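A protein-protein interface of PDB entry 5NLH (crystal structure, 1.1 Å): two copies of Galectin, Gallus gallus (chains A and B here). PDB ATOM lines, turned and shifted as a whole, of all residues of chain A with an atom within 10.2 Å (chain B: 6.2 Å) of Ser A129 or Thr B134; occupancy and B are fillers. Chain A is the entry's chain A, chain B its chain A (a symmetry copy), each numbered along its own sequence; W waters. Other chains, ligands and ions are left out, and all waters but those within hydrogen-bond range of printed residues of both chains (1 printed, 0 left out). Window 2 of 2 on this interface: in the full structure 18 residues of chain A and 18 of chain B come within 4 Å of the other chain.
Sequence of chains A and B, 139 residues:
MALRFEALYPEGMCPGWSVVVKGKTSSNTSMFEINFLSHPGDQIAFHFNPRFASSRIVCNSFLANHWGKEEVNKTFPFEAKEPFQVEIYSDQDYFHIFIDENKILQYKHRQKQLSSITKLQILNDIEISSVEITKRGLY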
ATOM      1  N   ARG A   4     -13.633 -38.296 -19.561  1.00  0.00           N
ATOM      2  CA  ARG A   4     -13.355 -37.088 -18.790  1.00  0.00           C
ATOM      3  C   ARG A   4     -13.723 -35.819 -19.567  1.00  0.00           C
ATOM      4  O   ARG A   4     -14.097 -34.819 -18.969  1.00  0.00           O
ATOM      5  CB  ARG A   4     -11.881 -37.035 -18.357  1.00  0.00           C
ATOM      6  CG  ARG A   4     -11.348 -38.301 -17.664  1.00  0.00           C
ATOM      7  CD  ARG A   4     -12.188 -38.757 -16.464  1.00  0.00           C
ATOM      8  NE  ARG A   4     -12.021 -37.931 -15.268  1.00  0.00           N
ATOM      9  CZ  ARG A   4     -11.124 -38.147 -14.308  1.00  0.00           C
ATOM     10  NH1 ARG A   4     -10.289 -39.172 -14.385  1.00  0.00           N
ATOM     11  NH2 ARG A   4     -11.083 -37.344 -13.250  1.00  0.00           N
ATOM     12  N   PHE A   5     -13.594 -35.855 -20.892  1.00  0.00           N
ATOM     13  CA  PHE A   5     -13.862 -34.682 -21.723  1.00  0.00           C
ATOM     14  C   PHE A   5     -14.118 -35.134 -23.154  1.00  0.00           C
ATOM     15  O   PHE A   5     -13.452 -36.049 -23.642  1.00  0.00           O
ATOM     16  CB  PHE A   5     -12.672 -33.713 -21.667  1.00  0.00           C
ATOM     17  CG  PHE A   5     -12.865 -32.460 -22.480  1.00  0.00           C
ATOM     18  CD1 PHE A   5     -13.437 -31.327 -21.920  1.00  0.00           C
ATOM     19  CD2 PHE A   5     -12.462 -32.400 -23.804  1.00  0.00           C
ATOM     20  CE1 PHE A   5     -13.603 -30.168 -22.676  1.00  0.00           C
ATOM     21  CE2 PHE A   5     -12.643 -31.250 -24.548  1.00  0.00           C
ATOM     22  CZ  PHE A   5     -13.203 -30.151 -23.984  1.00  0.00           C
ATOM     23  N   VAL A  20      -4.587 -28.453 -26.873  1.00  0.00           N
ATOM     24  CA  VAL A  20      -3.670 -28.341 -25.741  1.00  0.00           C
ATOM     25  C   VAL A  20      -4.438 -28.780 -24.509  1.00  0.00           C
ATOM     26  O   VAL A  20      -5.464 -28.188 -24.166  1.00  0.00           O
ATOM     27  CB  VAL A  20      -3.135 -26.901 -25.546  1.00  0.00           C
ATOM     28  CG1 VAL A  20      -2.155 -26.858 -24.397  1.00  0.00           C
ATOM     29  CG2 VAL A  20      -2.476 -26.389 -26.831  1.00  0.00           C
ATOM     30  N   VAL A  21      -3.940 -29.818 -23.853  1.00  0.00           N
ATOM     31  CA  VAL A  21      -4.563 -30.411 -22.673  1.00  0.00           C
ATOM     32  C   VAL A  21      -3.593 -30.241 -21.510  1.00  0.00           C
ATOM     33  O   VAL A  21      -2.435 -30.632 -21.598  1.00  0.00           O
ATOM     34  CB  VAL A  21      -4.839 -31.912 -22.887  1.00  0.00           C
ATOM     35  CG1 VAL A  21      -5.446 -32.537 -21.625  1.00  0.00           C
ATOM     36  CG2 VAL A  21      -5.750 -32.123 -24.082  1.00  0.00           C
ATOM     37  N   LYS A  22      -4.084 -29.631 -20.440  1.00  0.00           N
ATOM     38  CA  LYS A  22      -3.316 -29.486 -19.216  1.00  0.00           C
ATOM     39  C   LYS A  22      -4.015 -30.254 -18.120  1.00  0.00           C
ATOM     40  O   LYS A  22      -5.242 -30.257 -18.039  1.00  0.00           O
ATOM     41  CB  LYS A  22      -3.197 -28.020 -18.830  1.00  0.00           C
ATOM     42  CG  LYS A  22      -2.513 -27.185 -19.903  1.00  0.00           C
ATOM     43  CD  LYS A  22      -2.362 -25.725 -19.520  1.00  0.00           C
ATOM     44  CE  LYS A  22      -1.852 -24.904 -20.685  1.00  0.00           C
ATOM     45  NZ  LYS A  22      -1.597 -23.499 -20.312  1.00  0.00           N
ATOM     46  N   GLY A  23      -3.231 -30.924 -17.287  1.00  0.00           N
ATOM     47  CA  GLY A  23      -3.786 -31.662 -16.172  1.00  0.00           C
ATOM     48  C   GLY A  23      -2.720 -32.489 -15.504  1.00  0.00           C
ATOM     49  O   GLY A  23      -1.522 -32.250 -15.709  1.00  0.00           O
ATOM     50  N   LYS A  24      -3.141 -33.453 -14.694  1.00  0.00           N
ATOM     51  CA  LYS A  24      -2.219 -34.356 -14.020  1.00  0.00           C
ATOM     52  C   LYS A  24      -2.955 -35.668 -13.764  1.00  0.00           C
ATOM     53  O   LYS A  24      -4.192 -35.708 -13.748  1.00  0.00           O
ATOM     54  CB  LYS A  24      -1.696 -33.762 -12.698  1.00  0.00           C
ATOM     55  CG  LYS A  24      -2.754 -33.532 -11.637  1.00  0.00           C
ATOM     56  CD  LYS A  24      -2.115 -32.828 -10.449  1.00  0.00           C
ATOM     57  CE  LYS A  24      -3.096 -32.512  -9.343  1.00  0.00           C
ATOM     58  NZ  LYS A  24      -2.424 -31.789  -8.231  1.00  0.00           N
ATOM     59  N   THR A  25      -2.207 -36.747 -13.564  1.00  0.00           N
ATOM     60  CA  THR A  25      -2.817 -38.001 -13.174  1.00  0.00           C
ATOM     61  C   THR A  25      -3.085 -38.039 -11.684  1.00  0.00           C
ATOM     62  O   THR A  25      -2.483 -37.297 -10.898  1.00  0.00           O
ATOM     63  CB  THR A  25      -1.931 -39.197 -13.528  1.00  0.00           C
ATOM     64  OG1 THR A  25      -0.793 -39.222 -12.654  1.00  0.00           O
ATOM     65  CG2 THR A  25      -1.485 -39.157 -14.973  1.00  0.00           C
ATOM     66  N   GLU A  82       1.983 -34.963 -11.307  1.00  0.00           N
ATOM     67  CA  GLU A  82       2.619 -33.681 -11.602  1.00  0.00           C
ATOM     68  C   GLU A  82       1.965 -33.049 -12.832  1.00  0.00           C
ATOM     69  O   GLU A  82       1.776 -33.711 -13.850  1.00  0.00           O
ATOM     70  CB  GLU A  82       4.109 -33.873 -11.883  1.00  0.00           C
ATOM     71  CG  GLU A  82       4.917 -34.347 -10.694  1.00  0.00           C
ATOM     72  CD  GLU A  82       4.776 -33.449  -9.484  1.00  0.00           C
ATOM     73  OE1 GLU A  82       4.725 -32.223  -9.651  1.00  0.00           O
ATOM     74  OE2 GLU A  82       4.722 -33.981  -8.358  1.00  0.00           O
ATOM     75  N   PRO A  83       1.617 -31.762 -12.764  1.00  0.00           N
ATOM     76  CA  PRO A  83       0.981 -31.118 -13.912  1.00  0.00           C
ATOM     77  C   PRO A  83       1.829 -31.194 -15.159  1.00  0.00           C
ATOM     78  O   PRO A  83       3.054 -31.031 -15.105  1.00  0.00           O
ATOM     79  CB  PRO A  83       0.820 -29.671 -13.451  1.00  0.00           C
ATOM     80  CG  PRO A  83       0.676 -29.787 -11.981  1.00  0.00           C
ATOM     81  CD  PRO A  83       1.642 -30.872 -11.588  1.00  0.00           C
ATOM     82  N   PHE A  84       1.140 -31.428 -16.269  1.00  0.00           N
ATOM     83  CA  PHE A  84       1.746 -31.456 -17.586  1.00  0.00           C
ATOM     84  C   PHE A  84       0.905 -30.657 -18.566  1.00  0.00           C
ATOM     85  O   PHE A  84      -0.254 -30.316 -18.305  1.00  0.00           O
ATOM     86  CB  PHE A  84       1.903 -32.898 -18.105  1.00  0.00           C
ATOM     87  CG  PHE A  84       0.625 -33.708 -18.098  1.00  0.00           C
ATOM     88  CD1 PHE A  84      -0.376 -33.471 -19.028  1.00  0.00           C
ATOM     89  CD2 PHE A  84       0.431 -34.731 -17.175  1.00  0.00           C
ATOM     90  CE1 PHE A  84      -1.556 -34.214 -19.017  1.00  0.00           C
ATOM     91  CE2 PHE A  84      -0.731 -35.481 -17.172  1.00  0.00           C
ATOM     92  CZ  PHE A  84      -1.716 -35.229 -18.112  1.00  0.00           C
ATOM     93  N   GLN A  85       1.512 -30.368 -19.715  1.00  0.00           N
ATOM     94  CA  GLN A  85       0.829 -29.791 -20.867  1.00  0.00           C
ATOM     95  C   GLN A  85       1.130 -30.660 -22.076  1.00  0.00           C
ATOM     96  O   GLN A  85       2.284 -30.858 -22.416  1.00  0.00           O
ATOM     97  CB  GLN A  85       1.337 -28.370 -21.103  1.00  0.00           C
ATOM     98  CG  GLN A  85       0.821 -27.722 -22.349  1.00  0.00           C
ATOM     99  CD  GLN A  85       1.319 -26.316 -22.468  1.00  0.00           C
ATOM    100  OE1 GLN A  85       1.288 -25.559 -21.496  1.00  0.00           O
ATOM    101  NE2 GLN A  85       1.818 -25.958 -23.638  1.00  0.00           N
ATOM    102  N   VAL A  86       0.088 -31.167 -22.721  1.00  0.00           N
ATOM    103  CA  VAL A  86       0.239 -31.933 -23.949  1.00  0.00           C
ATOM    104  C   VAL A  86      -0.384 -31.120 -25.062  1.00  0.00           C
ATOM    105  O   VAL A  86      -1.549 -30.757 -24.981  1.00  0.00           O
ATOM    106  CB  VAL A  86      -0.485 -33.291 -23.870  1.00  0.00           C
ATOM    107  CG1 VAL A  86      -0.381 -34.037 -25.215  1.00  0.00           C
ATOM    108  CG2 VAL A  86       0.073 -34.147 -22.760  1.00  0.00           C
ATOM    109  N   ILE A 122     -11.161 -37.578 -24.238  1.00  0.00           N
ATOM    110  CA  ILE A 122     -10.106 -37.774 -23.260  1.00  0.00           C
ATOM    111  C   ILE A 122     -10.658 -38.687 -22.183  1.00  0.00           C
ATOM    112  O   ILE A 122     -11.711 -38.385 -21.616  1.00  0.00           O
ATOM    113  CB  ILE A 122      -9.656 -36.426 -22.647  1.00  0.00           C
ATOM    114  CG1 ILE A 122      -9.266 -35.431 -23.743  1.00  0.00           C
ATOM    115  CG2 ILE A 122      -8.538 -36.655 -21.623  1.00  0.00           C
ATOM    116  CD1 ILE A 122      -8.914 -34.043 -23.239  1.00  0.00           C
ATOM    117  N   ILE A 126      -6.851 -38.876 -15.840  1.00  0.00           N
ATOM    118  CA  ILE A 126      -6.348 -37.527 -16.014  1.00  0.00           C
ATOM    119  C   ILE A 126      -7.351 -36.591 -15.357  1.00  0.00           C
ATOM    120  O   ILE A 126      -8.559 -36.655 -15.625  1.00  0.00           O
ATOM    121  CB  ILE A 126      -6.091 -37.160 -17.505  1.00  0.00           C
ATOM    122  CG1 ILE A 126      -5.623 -35.711 -17.608  1.00  0.00           C
ATOM    123  CG2 ILE A 126      -7.321 -37.429 -18.384  1.00  0.00           C
ATOM    124  CD1 ILE A 126      -5.249 -35.268 -19.012  1.00  0.00           C
ATOM    125  N   GLU A 127      -6.827 -35.727 -14.488  1.00  0.00           N
ATOM    126  CA  GLU A 127      -7.579 -34.660 -13.853  1.00  0.00           C
ATOM    127  C   GLU A 127      -7.281 -33.411 -14.667  1.00  0.00           C
ATOM    128  O   GLU A 127      -6.180 -32.845 -14.614  1.00  0.00           O
ATOM    129  CB  GLU A 127      -7.122 -34.489 -12.404  1.00  0.00           C
ATOM    130  CG  GLU A 127      -7.358 -35.754 -11.591  1.00  0.00           C
ATOM    131  CD  GLU A 127      -6.882 -35.681 -10.173  1.00  0.00           C
ATOM    132  OE1 GLU A 127      -6.179 -34.721  -9.812  1.00  0.00           O
ATOM    133  OE2 GLU A 127      -7.212 -36.618  -9.432  1.00  0.00           O
ATOM    134  N   ILE A 128      -8.237 -33.027 -15.503  1.00  0.00           N
ATOM    135  CA  ILE A 128      -8.041 -31.950 -16.459  1.00  0.00           C
ATOM    136  C   ILE A 128      -8.144 -30.583 -15.789  1.00  0.00           C
ATOM    137  O   ILE A 128      -9.091 -30.309 -15.042  1.00  0.00           O
ATOM    138  CB  ILE A 128      -9.096 -32.073 -17.583  1.00  0.00           C
ATOM    139  CG1 ILE A 128      -8.876 -33.369 -18.370  1.00  0.00           C
ATOM    140  CG2 ILE A 128      -9.072 -30.863 -18.500  1.00  0.00           C
ATOM    141  CD1 ILE A 128     -10.011 -33.727 -19.321  1.00  0.00           C
ATOM    142  N   SER A 129      -7.194 -29.705 -16.099  1.00  0.00           N
ATOM    143  CA  SER A 129      -7.310 -28.302 -15.713  1.00  0.00           C
ATOM    144  C   SER A 129      -7.652 -27.385 -16.882  1.00  0.00           C
ATOM    145  O   SER A 129      -8.184 -26.300 -16.666  1.00  0.00           O
ATOM    146  CB  SER A 129      -6.033 -27.790 -15.033  1.00  0.00           C
ATOM    147  OG  SER A 129      -4.935 -27.828 -15.919  1.00  0.00           O
ATOM    148  N   SER A 130      -7.340 -27.783 -18.110  1.00  0.00           N
ATOM    149  CA  SER A 130      -7.666 -26.968 -19.276  1.00  0.00           C
ATOM    150  C   SER A 130      -7.665 -27.806 -20.554  1.00  0.00           C
ATOM    151  O   SER A 130      -6.812 -28.683 -20.715  1.00  0.00           O
ATOM    152  CB  SER A 130      -6.624 -25.854 -19.448  1.00  0.00           C
ATOM    153  OG  SER A 130      -6.918 -25.029 -20.566  1.00  0.00           O
ATOM    154  N   VAL A 131      -8.575 -27.486 -21.468  1.00  0.00           N
ATOM    155  CA  VAL A 131      -8.501 -27.968 -22.837  1.00  0.00           C
ATOM    156  C   VAL A 131      -8.688 -26.759 -23.749  1.00  0.00           C
ATOM    157  O   VAL A 131      -9.672 -26.027 -23.618  1.00  0.00           O
ATOM    158  CB  VAL A 131      -9.572 -29.031 -23.177  1.00  0.00           C
ATOM    159  CG1 VAL A 131      -9.393 -29.500 -24.631  1.00  0.00           C
ATOM    160  CG2 VAL A 131      -9.468 -30.205 -22.216  1.00  0.00           C
ATOM    161  N   GLU A 132      -7.740 -26.557 -24.660  1.00  0.00           N
ATOM    162  CA  GLU A 132      -7.817 -25.516 -25.674  1.00  0.00           C
ATOM    163  C   GLU A 132      -7.804 -26.169 -27.050  1.00  0.00           C
ATOM    164  O   GLU A 132      -6.971 -27.025 -27.300  1.00  0.00           O
ATOM    165  CB  GLU A 132      -6.619 -24.580 -25.540  1.00  0.00           C
ATOM    166  CG  GLU A 132      -6.551 -23.477 -26.578  1.00  0.00           C
ATOM    167  CD  GLU A 132      -5.166 -22.824 -26.712  1.00  0.00           C
ATOM    168  OE1 GLU A 132      -4.946 -22.116 -27.716  1.00  0.00           O
ATOM    169  OE2 GLU A 132      -4.284 -23.012 -25.839  1.00  0.00           O
ATOM    170  N   ILE A 133      -8.712 -25.747 -27.915  1.00  0.00           N
ATOM    171  CA  ILE A 133      -8.791 -26.241 -29.284  1.00  0.00           C
ATOM    172  C   ILE A 133      -8.729 -24.999 -30.172  1.00  0.00           C
ATOM    173  O   ILE A 133      -9.630 -24.169 -30.133  1.00  0.00           O
ATOM    174  CB  ILE A 133     -10.086 -27.036 -29.497  1.00  0.00           C
ATOM    175  CG1 ILE A 133     -10.114 -28.232 -28.528  1.00  0.00           C
ATOM    176  CG2 ILE A 133     -10.213 -27.479 -30.949  1.00  0.00           C
ATOM    177  CD1 ILE A 133     -11.407 -29.007 -28.496  1.00  0.00           C
ATOM    178  N   THR A 134      -7.651 -24.865 -30.948  1.00  0.00           N
ATOM    179  CA  THR A 134      -7.357 -23.614 -31.637  1.00  0.00           C
ATOM    180  C   THR A 134      -6.921 -23.859 -33.076  1.00  0.00           C
ATOM    181  O   THR A 134      -6.074 -24.718 -33.346  1.00  0.00           O
ATOM    182  CB  THR A 134      -6.263 -22.837 -30.883  1.00  0.00           C
ATOM    183  OG1 THR A 134      -6.746 -22.516 -29.579  1.00  0.00           O
ATOM    184  CG2 THR A 134      -5.891 -21.554 -31.583  1.00  0.00           C
ATOM    185  N   GLY B  16     -16.355 -21.823 -11.201  1.00  0.00           N
ATOM    186  CA  GLY B  16     -14.909 -21.758 -11.183  1.00  0.00           C
ATOM    187  C   GLY B  16     -14.203 -22.139 -12.462  1.00  0.00           C
ATOM    188  O   GLY B  16     -13.033 -22.491 -12.419  1.00  0.00           O
ATOM    189  N   TRP B  17     -14.911 -22.057 -13.582  1.00  0.00           N
ATOM    190  CA  TRP B  17     -14.336 -22.329 -14.897  1.00  0.00           C
ATOM    191  C   TRP B  17     -14.553 -21.133 -15.795  1.00  0.00           C
ATOM    192  O   TRP B  17     -15.566 -20.435 -15.700  1.00  0.00           O
ATOM    193  CB  TRP B  17     -14.988 -23.552 -15.546  1.00  0.00           C
ATOM    194  CG  TRP B  17     -14.650 -24.865 -14.900  1.00  0.00           C
ATOM    195  CD1 TRP B  17     -15.082 -25.334 -13.698  1.00  0.00           C
ATOM    196  CD2 TRP B  17     -13.798 -25.874 -15.440  1.00  0.00           C
ATOM    197  NE1 TRP B  17     -14.562 -26.580 -13.463  1.00  0.00           N
ATOM    198  CE2 TRP B  17     -13.767 -26.936 -14.521  1.00  0.00           C
ATOM    199  CE3 TRP B  17     -13.072 -25.989 -16.623  1.00  0.00           C
ATOM    200  CZ2 TRP B  17     -13.025 -28.094 -14.749  1.00  0.00           C
ATOM    201  CZ3 TRP B  17     -12.344 -27.126 -16.848  1.00  0.00           C
ATOM    202  CH2 TRP B  17     -12.312 -28.163 -15.914  1.00  0.00           C
ATOM    203  N   SER B  18     -13.595 -20.936 -16.689  1.00  0.00           N
ATOM    204  CA  SER B  18     -13.729 -20.009 -17.794  1.00  0.00           C
ATOM    205  C   SER B  18     -13.860 -20.743 -19.112  1.00  0.00           C
ATOM    206  O   SER B  18     -13.174 -21.748 -19.356  1.00  0.00           O
ATOM    207  CB  SER B  18     -12.505 -19.126 -17.918  1.00  0.00           C
ATOM    208  OG  SER B  18     -12.528 -18.104 -16.963  1.00  0.00           O
ATOM    209  N   VAL B  19     -14.715 -20.210 -19.973  1.00  0.00           N
ATOM    210  CA  VAL B  19     -14.811 -20.609 -21.365  1.00  0.00           C
ATOM    211  C   VAL B  19     -14.475 -19.386 -22.186  1.00  0.00           C
ATOM    212  O   VAL B  19     -15.087 -18.332 -22.007  1.00  0.00           O
ATOM    213  CB  VAL B  19     -16.221 -21.121 -21.717  1.00  0.00           C
ATOM    214  CG1 VAL B  19     -16.323 -21.420 -23.201  1.00  0.00           C
ATOM    215  CG2 VAL B  19     -16.538 -22.357 -20.914  1.00  0.00           C
ATOM    216  N   GLU B 132     -11.369 -22.348 -25.496  1.00  0.00           N
ATOM    217  CA  GLU B 132     -10.597 -22.760 -24.333  1.00  0.00           C
ATOM    218  C   GLU B 132     -11.546 -22.953 -23.158  1.00  0.00           C
ATOM    219  O   GLU B 132     -12.373 -22.092 -22.906  1.00  0.00           O
ATOM    220  CB  GLU B 132      -9.571 -21.683 -23.991  1.00  0.00           C
ATOM    221  CG  GLU B 132      -8.734 -21.968 -22.759  1.00  0.00           C
ATOM    222  CD  GLU B 132      -8.029 -20.731 -22.179  1.00  0.00           C
ATOM    223  OE1 GLU B 132      -7.557 -20.812 -21.027  1.00  0.00           O
ATOM    224  OE2 GLU B 132      -7.947 -19.671 -22.846  1.00  0.00           O
ATOM    225  N   ILE B 133     -11.401 -24.066 -22.456  1.00  0.00           N
ATOM    226  CA  ILE B 133     -12.200 -24.367 -21.275  1.00  0.00           C
ATOM    227  C   ILE B 133     -11.195 -24.642 -20.158  1.00  0.00           C
ATOM    228  O   ILE B 133     -10.445 -25.610 -20.229  1.00  0.00           O
ATOM    229  CB  ILE B 133     -13.115 -25.571 -21.535  1.00  0.00           C
ATOM    230  CG1 ILE B 133     -14.056 -25.251 -22.710  1.00  0.00           C
ATOM    231  CG2 ILE B 133     -13.887 -25.941 -20.275  1.00  0.00           C
ATOM    232  CD1 ILE B 133     -14.894 -26.405 -23.200  1.00  0.00           C
ATOM    233  N   THR B 134     -11.164 -23.774 -19.146  1.00  0.00           N
ATOM    234  CA  THR B 134     -10.086 -23.784 -18.163  1.00  0.00           C
ATOM    235  C   THR B 134     -10.623 -23.630 -16.745  1.00  0.00           C
ATOM    236  O   THR B 134     -11.457 -22.759 -16.472  1.00  0.00           O
ATOM    237  CB  THR B 134      -9.079 -22.660 -18.468  1.00  0.00           C
ATOM    238  OG1 THR B 134      -8.504 -22.898 -19.752  1.00  0.00           O
ATOM    239  CG2 THR B 134      -7.968 -22.601 -17.450  1.00  0.00           C
ATOM    240  N   LYS B 135     -10.126 -24.467 -15.849  1.00  0.00           N
ATOM    241  CA  LYS B 135     -10.463 -24.383 -14.435  1.00  0.00           C
ATOM    242  C   LYS B 135      -9.663 -23.248 -13.811  1.00  0.00           C
ATOM    243  O   LYS B 135      -8.436 -23.287 -13.814  1.00  0.00           O
ATOM    244  CB  LYS B 135     -10.169 -25.729 -13.755  1.00  0.00           C
ATOM    245  CG  LYS B 135     -10.680 -25.815 -12.331  1.00  0.00           C
ATOM    246  CD  LYS B 135     -10.065 -26.963 -11.561  1.00  0.00           C
ATOM    247  CE  LYS B 135     -10.381 -28.306 -12.195  1.00  0.00           C
ATOM    248  NZ  LYS B 135      -9.762 -29.428 -11.428  1.00  0.00           N
ATOM    249  N   ARG B 136     -10.342 -22.237 -13.271  1.00  0.00           N
ATOM    250  CA  ARG B 136      -9.678 -21.050 -12.718  1.00  0.00           C
ATOM    251  C   ARG B 136      -9.499 -21.043 -11.225  1.00  0.00           C
ATOM    252  O   ARG B 136      -8.545 -20.458 -10.715  1.00  0.00           O
ATOM    253  CB  ARG B 136     -10.507 -19.806 -12.973  1.00  0.00           C
ATOM    254  CG  ARG B 136     -10.764 -19.516 -14.386  1.00  0.00           C
ATOM    255  CD  ARG B 136      -9.494 -19.153 -15.109  1.00  0.00           C
ATOM    256  NE  ARG B 136      -9.801 -18.483 -16.369  1.00  0.00           N
ATOM    257  CZ  ARG B 136      -8.923 -18.311 -17.351  1.00  0.00           C
ATOM    258  NH1 ARG B 136      -7.686 -18.764 -17.219  1.00  0.00           N
ATOM    259  NH2 ARG B 136      -9.282 -17.691 -18.464  1.00  0.00           N
ATOM    260  N   GLY B 137     -10.475 -21.590 -10.519  1.00  0.00           N
ATOM    261  CA  GLY B 137     -10.597 -21.329  -9.100  1.00  0.00           C
ATOM    262  C   GLY B 137     -11.711 -20.337  -8.827  1.00  0.00           C
ATOM    263  O   GLY B 137     -12.311 -19.780  -9.754  1.00  0.00           O
HETATM  264  O   HOH W   1     -10.329 -31.694 -13.155  1.00  0.00           O
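The backbone carbonyl oxygen (O) of Ser A129 sits at hydrogen-bond distance from the backbone NH (N) of Lys B135, 2.8 Å away.
OG1 of Thr B134 sits at hydrogen-bond distance from OG of Ser A130.
The backbone carbonyl oxygen of Val A131 sits at hydrogen-bond distance from the backbone NH of Ile B133 (2.9 Å).
O of Lys A22 sits at hydrogen-bond distance from N of Ser A129, at 2.8 Å.
The backbone carbonyl oxygen (O) of Ser A130 lies within hydrogen-bond range of the backbone NH (N) of Lys A22 (2.9 Å).
O of Thr B134 lies within hydrogen-bond range of N of Ser B18.
The side-chain carboxylate of Glu B132 lies within hydrogen-bond range of the side-chain hydroxyl of Thr B134.
Among the printed residues, merely in contact across the chains: Ser A130 with Ile B133 (3.2 Å), Val A131 with Glu B132 (3.5 Å), Ser A129 with Thr B134 (3.5 Å), Ile A128 with Lys B135 (3.7 Å) and Ile A128 with Trp B17 (3.97 Å).
Ser A129 touches two residues of chain B.
Printed residues of chain A within 4 Å of Thr B134: Ser A129 (3.5 Å) and Ser A130 (2.8 Å).
Trp B17 touches just one residue of chain A: Ile A128 (3.97 Å).
No residue of chain A comes within 4 Å of Ser B18.
Of the printed residues of chain A, Lys B135 touches Ile A128 and Ser A129.
Printed residues of chain B within 4 Å of Val A131: Glu B132 (3.5 Å) and Ile B133 (2.9 Å).
Printed residues of chain A within 4 Å of Glu B132: Val A131.
Val A20 touches none of the printed residues of chain B.
The nearest residue of chain B that does not touch Ser A129 is Trp B17 (4.2 Å).
The nearest printed residue of chain A that does not touch Thr B134 is Val A131 (4.9 Å).
Of the 10 printed residues of chain B, 5 touch a printed residue of chain A.
Printed residues of chain B that touch a printed residue of chain A: Trp B17, Glu B132, Ile B133, Thr B134 and Lys B135.
Hydrophobic or aromatic side chains of chain B that line the printed part of chain A: Trp B17.
Among the printed residues, 8 pairs touch across the chains.
Positions printed for both chains: 132, 133 and 134.
Of the 8 pairs that touch across the chains among the printed residues, none has its exchanged pair printed and touching as well.
Water W1 bridges O of Ile A128 (2.6 Å) and NZ of Lys B135 (2.9 Å).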
